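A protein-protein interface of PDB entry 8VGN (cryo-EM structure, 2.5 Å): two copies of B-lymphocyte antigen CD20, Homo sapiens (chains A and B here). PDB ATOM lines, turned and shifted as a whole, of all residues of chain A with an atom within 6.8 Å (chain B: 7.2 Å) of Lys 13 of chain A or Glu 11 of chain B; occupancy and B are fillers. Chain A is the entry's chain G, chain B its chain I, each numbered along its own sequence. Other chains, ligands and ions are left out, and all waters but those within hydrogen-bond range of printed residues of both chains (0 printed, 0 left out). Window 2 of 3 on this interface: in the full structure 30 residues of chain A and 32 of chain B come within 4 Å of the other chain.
The side-chain carboxylate (OE2) of Glu 11 of chain A is in salt-bridge range of the side-chain amino group (NZ) of Lys 13 of chain B (2.8 Å). OE2 of Glu 11 of chain B is in salt-bridge range of NZ of Lys 13 of chain A (2.8 Å).
The side-chain hydroxyl of Thr 14 of chain A sits at hydrogen-bond distance from the side-chain carboxylate of Glu 11 of chain A (2.6 Å). OE1 of Glu 11 of chain B is in hydrogen-bond range of OG1 of Thr 14 of chain B (2.6 Å).
Thr 14 of chain B touches Lys 13 of chain A (OG1 to NZ, 3.8 Å). OG1 of Thr 14 of chain A touches NZ of Lys 13 of chain B, at 3.8 Å. Thr 14 of chain A touches Ala 17 of chain B (CG2 to CB, 3.6 Å). Ala 17 of chain A touches Thr 14 of chain B (CB to CG2, 3.6 Å).
Of the printed residues of chain B, Glu 11 of chain A touches Lys 13. Of chain B, only Glu 11 (2.8 Å) and Thr 14 (3.8 Å) come within 4 Å of Lys 13 of chain A. Of the printed residues of chain B, Ala 17 of chain A touches Thr 14 (3.6 Å). Of chain A, only Lys 13 comes within 4 Å of Glu 11 of chain B. Of the printed residues of chain A, Thr 14 of chain B touches Lys 13 and Ala 17. Leu 15 of chain B touches none of the printed residues of chain A. Printed residues of chain A within 4 Å of Ala 17 of chain B: Thr 14. The nearest residue of chain A that does not touch Glu 11 of chain B is Leu 64 of chain A (6.1 Å). The nearest printed residue of chain B that does not touch Glu 11 of chain A is Leu 64 of chain B (6.1 Å).
Of the 12 printed residues of chain B, 4 touch a printed residue of chain A. Of the 13 printed residues of chain A, 4 touch a printed residue of chain B. Printed residues of chain A that touch a printed residue of chain B: Glu 11, Lys 13, Thr 14 and Ala 17. Hydrophobic or aromatic side chains of chain A that line the printed part of chain B: Ala 17. Among the printed residues, 6 pairs touch across the chains.
Glu 11 of chain A touches Lys 13 of chain B, and with the chains exchanged Lys 13 of chain A touches Glu 11 of chain B. Lys 13 of chain A touches Thr 14 of chain B, and with the chains exchanged Thr 14 of chain A touches Lys 13 of chain B. Thr 14 of chain A touches Ala 17 of chain B, and with the chains exchanged Ala 17 of chain A touches Thr 14 of chain B. Of the 6 pairs that touch across the chains among the printed residues, 6 have their exchanged pair printed and touching as well.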
ATOM      1  N   ARG A  10      16.452 -16.763  -3.314  1.00  0.00           N
ATOM      2  CA  ARG A  10      15.261 -17.487  -3.752  1.00  0.00           C
ATOM      3  C   ARG A  10      14.429 -16.701  -4.762  1.00  0.00           C
ATOM      4  O   ARG A  10      13.806 -17.299  -5.647  1.00  0.00           O
ATOM      5  CB  ARG A  10      14.414 -17.847  -2.533  1.00  0.00           C
ATOM      6  CG  ARG A  10      13.109 -18.548  -2.842  1.00  0.00           C
ATOM      7  CD  ARG A  10      12.386 -18.899  -1.554  1.00  0.00           C
ATOM      8  NE  ARG A  10      11.067 -19.469  -1.793  1.00  0.00           N
ATOM      9  CZ  ARG A  10      10.164 -19.683  -0.847  1.00  0.00           C
ATOM     10  NH1 ARG A  10      10.421 -19.426   0.425  1.00  0.00           N
ATOM     11  NH2 ARG A  10       8.977 -20.181  -1.183  1.00  0.00           N
ATOM     12  N   GLU A  11      14.405 -15.372  -4.650  1.00  0.00           N
ATOM     13  CA  GLU A  11      13.531 -14.514  -5.450  1.00  0.00           C
ATOM     14  C   GLU A  11      13.816 -14.564  -6.949  1.00  0.00           C
ATOM     15  O   GLU A  11      14.016 -13.521  -7.577  1.00  0.00           O
ATOM     16  CB  GLU A  11      13.639 -13.072  -4.959  1.00  0.00           C
ATOM     17  CG  GLU A  11      12.815 -12.790  -3.723  1.00  0.00           C
ATOM     18  CD  GLU A  11      11.368 -12.491  -4.050  1.00  0.00           C
ATOM     19  OE1 GLU A  11      11.077 -11.356  -4.481  1.00  0.00           O
ATOM     20  OE2 GLU A  11      10.521 -13.392  -3.880  1.00  0.00           O
ATOM     21  N   SER A  12      13.859 -15.765  -7.527  1.00  0.00           N
ATOM     22  CA  SER A  12      14.319 -15.923  -8.904  1.00  0.00           C
ATOM     23  C   SER A  12      13.402 -15.236  -9.911  1.00  0.00           C
ATOM     24  O   SER A  12      13.869 -14.758 -10.947  1.00  0.00           O
ATOM     25  CB  SER A  12      14.444 -17.406  -9.241  1.00  0.00           C
ATOM     26  OG  SER A  12      15.290 -18.066  -8.317  1.00  0.00           O
ATOM     27  N   LYS A  13      12.102 -15.176  -9.630  1.00  0.00           N
ATOM     28  CA  LYS A  13      11.189 -14.420 -10.483  1.00  0.00           C
ATOM     29  C   LYS A  13      11.505 -12.930 -10.453  1.00  0.00           C
ATOM     30  O   LYS A  13      11.723 -12.303 -11.491  1.00  0.00           O
ATOM     31  CB  LYS A  13       9.748 -14.674 -10.038  1.00  0.00           C
ATOM     32  CG  LYS A  13       9.327 -16.136 -10.074  1.00  0.00           C
ATOM     33  CD  LYS A  13       9.532 -16.764 -11.437  1.00  0.00           C
ATOM     34  CE  LYS A  13       8.745 -16.023 -12.494  1.00  0.00           C
ATOM     35  NZ  LYS A  13       7.288 -16.246 -12.305  1.00  0.00           N
ATOM     36  N   THR A  14      11.535 -12.349  -9.259  1.00  0.00           N
ATOM     37  CA  THR A  14      11.812 -10.924  -9.115  1.00  0.00           C
ATOM     38  C   THR A  14      13.163 -10.547  -9.710  1.00  0.00           C
ATOM     39  O   THR A  14      13.273  -9.577 -10.463  1.00  0.00           O
ATOM     40  CB  THR A  14      11.747 -10.539  -7.642  1.00  0.00           C
ATOM     41  OG1 THR A  14      10.646 -11.213  -7.026  1.00  0.00           O
ATOM     42  CG2 THR A  14      11.551  -9.051  -7.498  1.00  0.00           C
ATOM     43  N   LEU A  15      14.202 -11.317  -9.393  1.00  0.00           N
ATOM     44  CA  LEU A  15      15.550 -10.991  -9.846  1.00  0.00           C
ATOM     45  C   LEU A  15      15.732 -11.187 -11.344  1.00  0.00           C
ATOM     46  O   LEU A  15      16.416 -10.391 -11.991  1.00  0.00           O
ATOM     47  CB  LEU A  15      16.565 -11.834  -9.083  1.00  0.00           C
ATOM     48  CG  LEU A  15      16.685 -11.505  -7.605  1.00  0.00           C
ATOM     49  CD1 LEU A  15      17.564 -12.517  -6.915  1.00  0.00           C
ATOM     50  CD2 LEU A  15      17.237 -10.112  -7.445  1.00  0.00           C
ATOM     51  N   GLY A  16      15.159 -12.244 -11.913  1.00  0.00           N
ATOM     52  CA  GLY A  16      15.229 -12.414 -13.357  1.00  0.00           C
ATOM     53  C   GLY A  16      14.575 -11.294 -14.143  1.00  0.00           C
ATOM     54  O   GLY A  16      15.100 -10.856 -15.166  1.00  0.00           O
ATOM     55  N   ALA A  17      13.428 -10.808 -13.674  1.00  0.00           N
ATOM     56  CA  ALA A  17      12.765  -9.683 -14.327  1.00  0.00           C
ATOM     57  C   ALA A  17      13.579  -8.401 -14.235  1.00  0.00           C
ATOM     58  O   ALA A  17      13.632  -7.624 -15.193  1.00  0.00           O
ATOM     59  CB  ALA A  17      11.384  -9.470 -13.719  1.00  0.00           C
ATOM     60  N   VAL A  18      14.191  -8.147 -13.082  1.00  0.00           N
ATOM     61  CA  VAL A  18      15.130  -7.039 -12.933  1.00  0.00           C
ATOM     62  C   VAL A  18      16.257  -7.108 -13.959  1.00  0.00           C
ATOM     63  O   VAL A  18      16.631  -6.093 -14.555  1.00  0.00           O
ATOM     64  CB  VAL A  18      15.680  -7.017 -11.497  1.00  0.00           C
ATOM     65  CG1 VAL A  18      16.871  -6.111 -11.404  1.00  0.00           C
ATOM     66  CG2 VAL A  18      14.612  -6.570 -10.543  1.00  0.00           C
ATOM     67  N   LEU A  63      16.532 -17.374 -15.618  1.00  0.00           N
ATOM     68  CA  LEU A  63      16.094 -17.849 -14.312  1.00  0.00           C
ATOM     69  C   LEU A  63      14.677 -17.432 -13.956  1.00  0.00           C
ATOM     70  O   LEU A  63      14.208 -17.798 -12.875  1.00  0.00           O
ATOM     71  CB  LEU A  63      17.075 -17.411 -13.221  1.00  0.00           C
ATOM     72  CG  LEU A  63      17.402 -15.958 -12.894  1.00  0.00           C
ATOM     73  CD1 LEU A  63      16.842 -15.585 -11.542  1.00  0.00           C
ATOM     74  CD2 LEU A  63      18.904 -15.753 -12.912  1.00  0.00           C
ATOM     75  N   LEU A  64      13.986 -16.680 -14.811  1.00  0.00           N
ATOM     76  CA  LEU A  64      12.529 -16.631 -14.739  1.00  0.00           C
ATOM     77  C   LEU A  64      11.899 -17.996 -14.971  1.00  0.00           C
ATOM     78  O   LEU A  64      10.918 -18.356 -14.311  1.00  0.00           O
ATOM     79  CB  LEU A  64      11.982 -15.634 -15.750  1.00  0.00           C
ATOM     80  CG  LEU A  64      12.244 -14.181 -15.395  1.00  0.00           C
ATOM     81  CD1 LEU A  64      11.407 -13.268 -16.271  1.00  0.00           C
ATOM     82  CD2 LEU A  64      11.927 -13.984 -13.960  1.00  0.00           C
ATOM     83  N   ALA A  65      12.436 -18.767 -15.916  1.00  0.00           N
ATOM     84  CA  ALA A  65      12.009 -20.149 -16.137  1.00  0.00           C
ATOM     85  C   ALA A  65      12.628 -21.100 -15.110  1.00  0.00           C
ATOM     86  O   ALA A  65      13.391 -22.009 -15.437  1.00  0.00           O
ATOM     87  CB  ALA A  65      12.348 -20.573 -17.559  1.00  0.00           C
ATOM     88  N   ALA A  66      12.301 -20.844 -13.844  1.00  0.00           N
ATOM     89  CA  ALA A  66      12.962 -21.446 -12.684  1.00  0.00           C
ATOM     90  C   ALA A  66      14.430 -21.051 -12.610  1.00  0.00           C
ATOM     91  O   ALA A  66      15.314 -21.893 -12.750  1.00  0.00           O
ATOM     92  CB  ALA A  66      12.817 -22.965 -12.695  1.00  0.00           C
ATOM     93  N   MET B   9      -2.376  -9.441 -13.628  1.00  0.00           N
ATOM     94  CA  MET B   9      -2.134 -10.876 -13.694  1.00  0.00           C
ATOM     95  C   MET B   9      -1.584 -11.342 -12.340  1.00  0.00           C
ATOM     96  O   MET B   9      -1.181 -10.523 -11.517  1.00  0.00           O
ATOM     97  CB  MET B   9      -1.182 -11.198 -14.856  1.00  0.00           C
ATOM     98  CG  MET B   9      -0.786 -12.663 -15.016  1.00  0.00           C
ATOM     99  SD  MET B   9      -0.045 -13.030 -16.619  1.00  0.00           S
ATOM    100  CE  MET B   9       1.474 -12.089 -16.531  1.00  0.00           C
ATOM    101  N   ARG B  10      -1.609 -12.657 -12.108  1.00  0.00           N
ATOM    102  CA  ARG B  10      -1.106 -13.231 -10.863  1.00  0.00           C
ATOM    103  C   ARG B  10       0.344 -12.847 -10.579  1.00  0.00           C
ATOM    104  O   ARG B  10       0.727 -12.701  -9.412  1.00  0.00           O
ATOM    105  CB  ARG B  10      -1.250 -14.751 -10.914  1.00  0.00           C
ATOM    106  CG  ARG B  10      -0.704 -15.488  -9.711  1.00  0.00           C
ATOM    107  CD  ARG B  10      -0.952 -16.979  -9.853  1.00  0.00           C
ATOM    108  NE  ARG B  10      -0.342 -17.750  -8.777  1.00  0.00           N
ATOM    109  CZ  ARG B  10      -0.248 -19.072  -8.766  1.00  0.00           C
ATOM    110  NH1 ARG B  10      -0.755 -19.809  -9.742  1.00  0.00           N
ATOM    111  NH2 ARG B  10       0.357 -19.671  -7.745  1.00  0.00           N
ATOM    112  N   GLU B  11       1.161 -12.678 -11.620  1.00  0.00           N
ATOM    113  CA  GLU B  11       2.600 -12.462 -11.483  1.00  0.00           C
ATOM    114  C   GLU B  11       2.970 -11.173 -10.753  1.00  0.00           C
ATOM    115  O   GLU B  11       3.748 -10.368 -11.272  1.00  0.00           O
ATOM    116  CB  GLU B  11       3.253 -12.469 -12.863  1.00  0.00           C
ATOM    117  CG  GLU B  11       3.494 -13.859 -13.412  1.00  0.00           C
ATOM    118  CD  GLU B  11       4.773 -14.472 -12.888  1.00  0.00           C
ATOM    119  OE1 GLU B  11       5.857 -14.108 -13.387  1.00  0.00           O
ATOM    120  OE2 GLU B  11       4.696 -15.318 -11.972  1.00  0.00           O
ATOM    121  N   SER B  12       2.405 -10.955  -9.565  1.00  0.00           N
ATOM    122  CA  SER B  12       2.544  -9.669  -8.888  1.00  0.00           C
ATOM    123  C   SER B  12       3.986  -9.366  -8.498  1.00  0.00           C
ATOM    124  O   SER B  12       4.393  -8.201  -8.481  1.00  0.00           O
ATOM    125  CB  SER B  12       1.650  -9.635  -7.652  1.00  0.00           C
ATOM    126  OG  SER B  12       0.305  -9.918  -7.992  1.00  0.00           O
ATOM    127  N   LYS B  13       4.774 -10.390  -8.178  1.00  0.00           N
ATOM    128  CA  LYS B  13       6.196 -10.185  -7.921  1.00  0.00           C
ATOM    129  C   LYS B  13       6.925  -9.708  -9.171  1.00  0.00           C
ATOM    130  O   LYS B  13       7.596  -8.675  -9.161  1.00  0.00           O
ATOM    131  CB  LYS B  13       6.815 -11.483  -7.404  1.00  0.00           C
ATOM    132  CG  LYS B  13       6.179 -12.020  -6.130  1.00  0.00           C
ATOM    133  CD  LYS B  13       6.180 -11.003  -5.009  1.00  0.00           C
ATOM    134  CE  LYS B  13       7.591 -10.567  -4.681  1.00  0.00           C
ATOM    135  NZ  LYS B  13       8.342 -11.679  -4.044  1.00  0.00           N
ATOM    136  N   THR B  14       6.797 -10.456 -10.261  1.00  0.00           N
ATOM    137  CA  THR B  14       7.461 -10.099 -11.509  1.00  0.00           C
ATOM    138  C   THR B  14       7.036  -8.721 -12.003  1.00  0.00           C
ATOM    139  O   THR B  14       7.877  -7.894 -12.368  1.00  0.00           O
ATOM    140  CB  THR B  14       7.168 -11.159 -12.563  1.00  0.00           C
ATOM    141  OG1 THR B  14       7.228 -12.454 -11.957  1.00  0.00           O
ATOM    142  CG2 THR B  14       8.187 -11.092 -13.671  1.00  0.00           C
ATOM    143  N   LEU B  15       5.733  -8.451 -12.005  1.00  0.00           N
ATOM    144  CA  LEU B  15       5.223  -7.191 -12.539  1.00  0.00           C
ATOM    145  C   LEU B  15       5.563  -5.997 -11.658  1.00  0.00           C
ATOM    146  O   LEU B  15       5.870  -4.920 -12.173  1.00  0.00           O
ATOM    147  CB  LEU B  15       3.715  -7.287 -12.725  1.00  0.00           C
ATOM    148  CG  LEU B  15       3.265  -8.244 -13.817  1.00  0.00           C
ATOM    149  CD1 LEU B  15       1.766  -8.400 -13.789  1.00  0.00           C
ATOM    150  CD2 LEU B  15       3.730  -7.730 -15.155  1.00  0.00           C
ATOM    151  N   GLY B  16       5.495  -6.149 -10.339  1.00  0.00           N
ATOM    152  CA  GLY B  16       5.913  -5.065  -9.463  1.00  0.00           C
ATOM    153  C   GLY B  16       7.372  -4.676  -9.614  1.00  0.00           C
ATOM    154  O   GLY B  16       7.711  -3.494  -9.599  1.00  0.00           O
ATOM    155  N   ALA B  17       8.253  -5.662  -9.773  1.00  0.00           N
ATOM    156  CA  ALA B  17       9.666  -5.378 -10.003  1.00  0.00           C
ATOM    157  C   ALA B  17       9.904  -4.661 -11.324  1.00  0.00           C
ATOM    158  O   ALA B  17      10.729  -3.748 -11.403  1.00  0.00           O
ATOM    159  CB  ALA B  17      10.470  -6.671  -9.957  1.00  0.00           C
ATOM    160  N   LEU B  63       2.790  -3.568  -5.066  1.00  0.00           N
ATOM    161  CA  LEU B  63       2.264  -4.916  -5.243  1.00  0.00           C
ATOM    162  C   LEU B  63       3.329  -5.998  -5.180  1.00  0.00           C
ATOM    163  O   LEU B  63       2.983  -7.177  -5.303  1.00  0.00           O
ATOM    164  CB  LEU B  63       1.468  -5.020  -6.548  1.00  0.00           C
ATOM    165  CG  LEU B  63       2.050  -4.747  -7.931  1.00  0.00           C
ATOM    166  CD1 LEU B  63       2.127  -6.028  -8.730  1.00  0.00           C
ATOM    167  CD2 LEU B  63       1.195  -3.728  -8.661  1.00  0.00           C
ATOM    168  N   LEU B  64       4.602  -5.646  -5.007  1.00  0.00           N
ATOM    169  CA  LEU B  64       5.574  -6.617  -4.509  1.00  0.00           C
ATOM    170  C   LEU B  64       5.212  -7.122  -3.119  1.00  0.00           C
ATOM    171  O   LEU B  64       5.368  -8.312  -2.826  1.00  0.00           O
ATOM    172  CB  LEU B  64       6.967  -6.007  -4.490  1.00  0.00           C
ATOM    173  CG  LEU B  64       7.580  -5.812  -5.864  1.00  0.00           C
ATOM    174  CD1 LEU B  64       9.061  -5.500  -5.741  1.00  0.00           C
ATOM    175  CD2 LEU B  64       7.356  -7.043  -6.660  1.00  0.00           C
ATOM    176  N   ILE B 174      -3.147  -4.672 -14.795  1.00  0.00           N
ATOM    177  CA  ILE B 174      -3.367  -4.859 -13.367  1.00  0.00           C
ATOM    178  C   ILE B 174      -4.701  -4.264 -12.933  1.00  0.00           C
ATOM    179  O   ILE B 174      -5.494  -4.920 -12.259  1.00  0.00           O
ATOM    180  CB  ILE B 174      -2.203  -4.257 -12.550  1.00  0.00           C
ATOM    181  CG1 ILE B 174      -0.947  -5.116 -12.696  1.00  0.00           C
ATOM    182  CG2 ILE B 174      -2.588  -4.127 -11.097  1.00  0.00           C
ATOM    183  CD1 ILE B 174       0.324  -4.393 -12.340  1.00  0.00           C
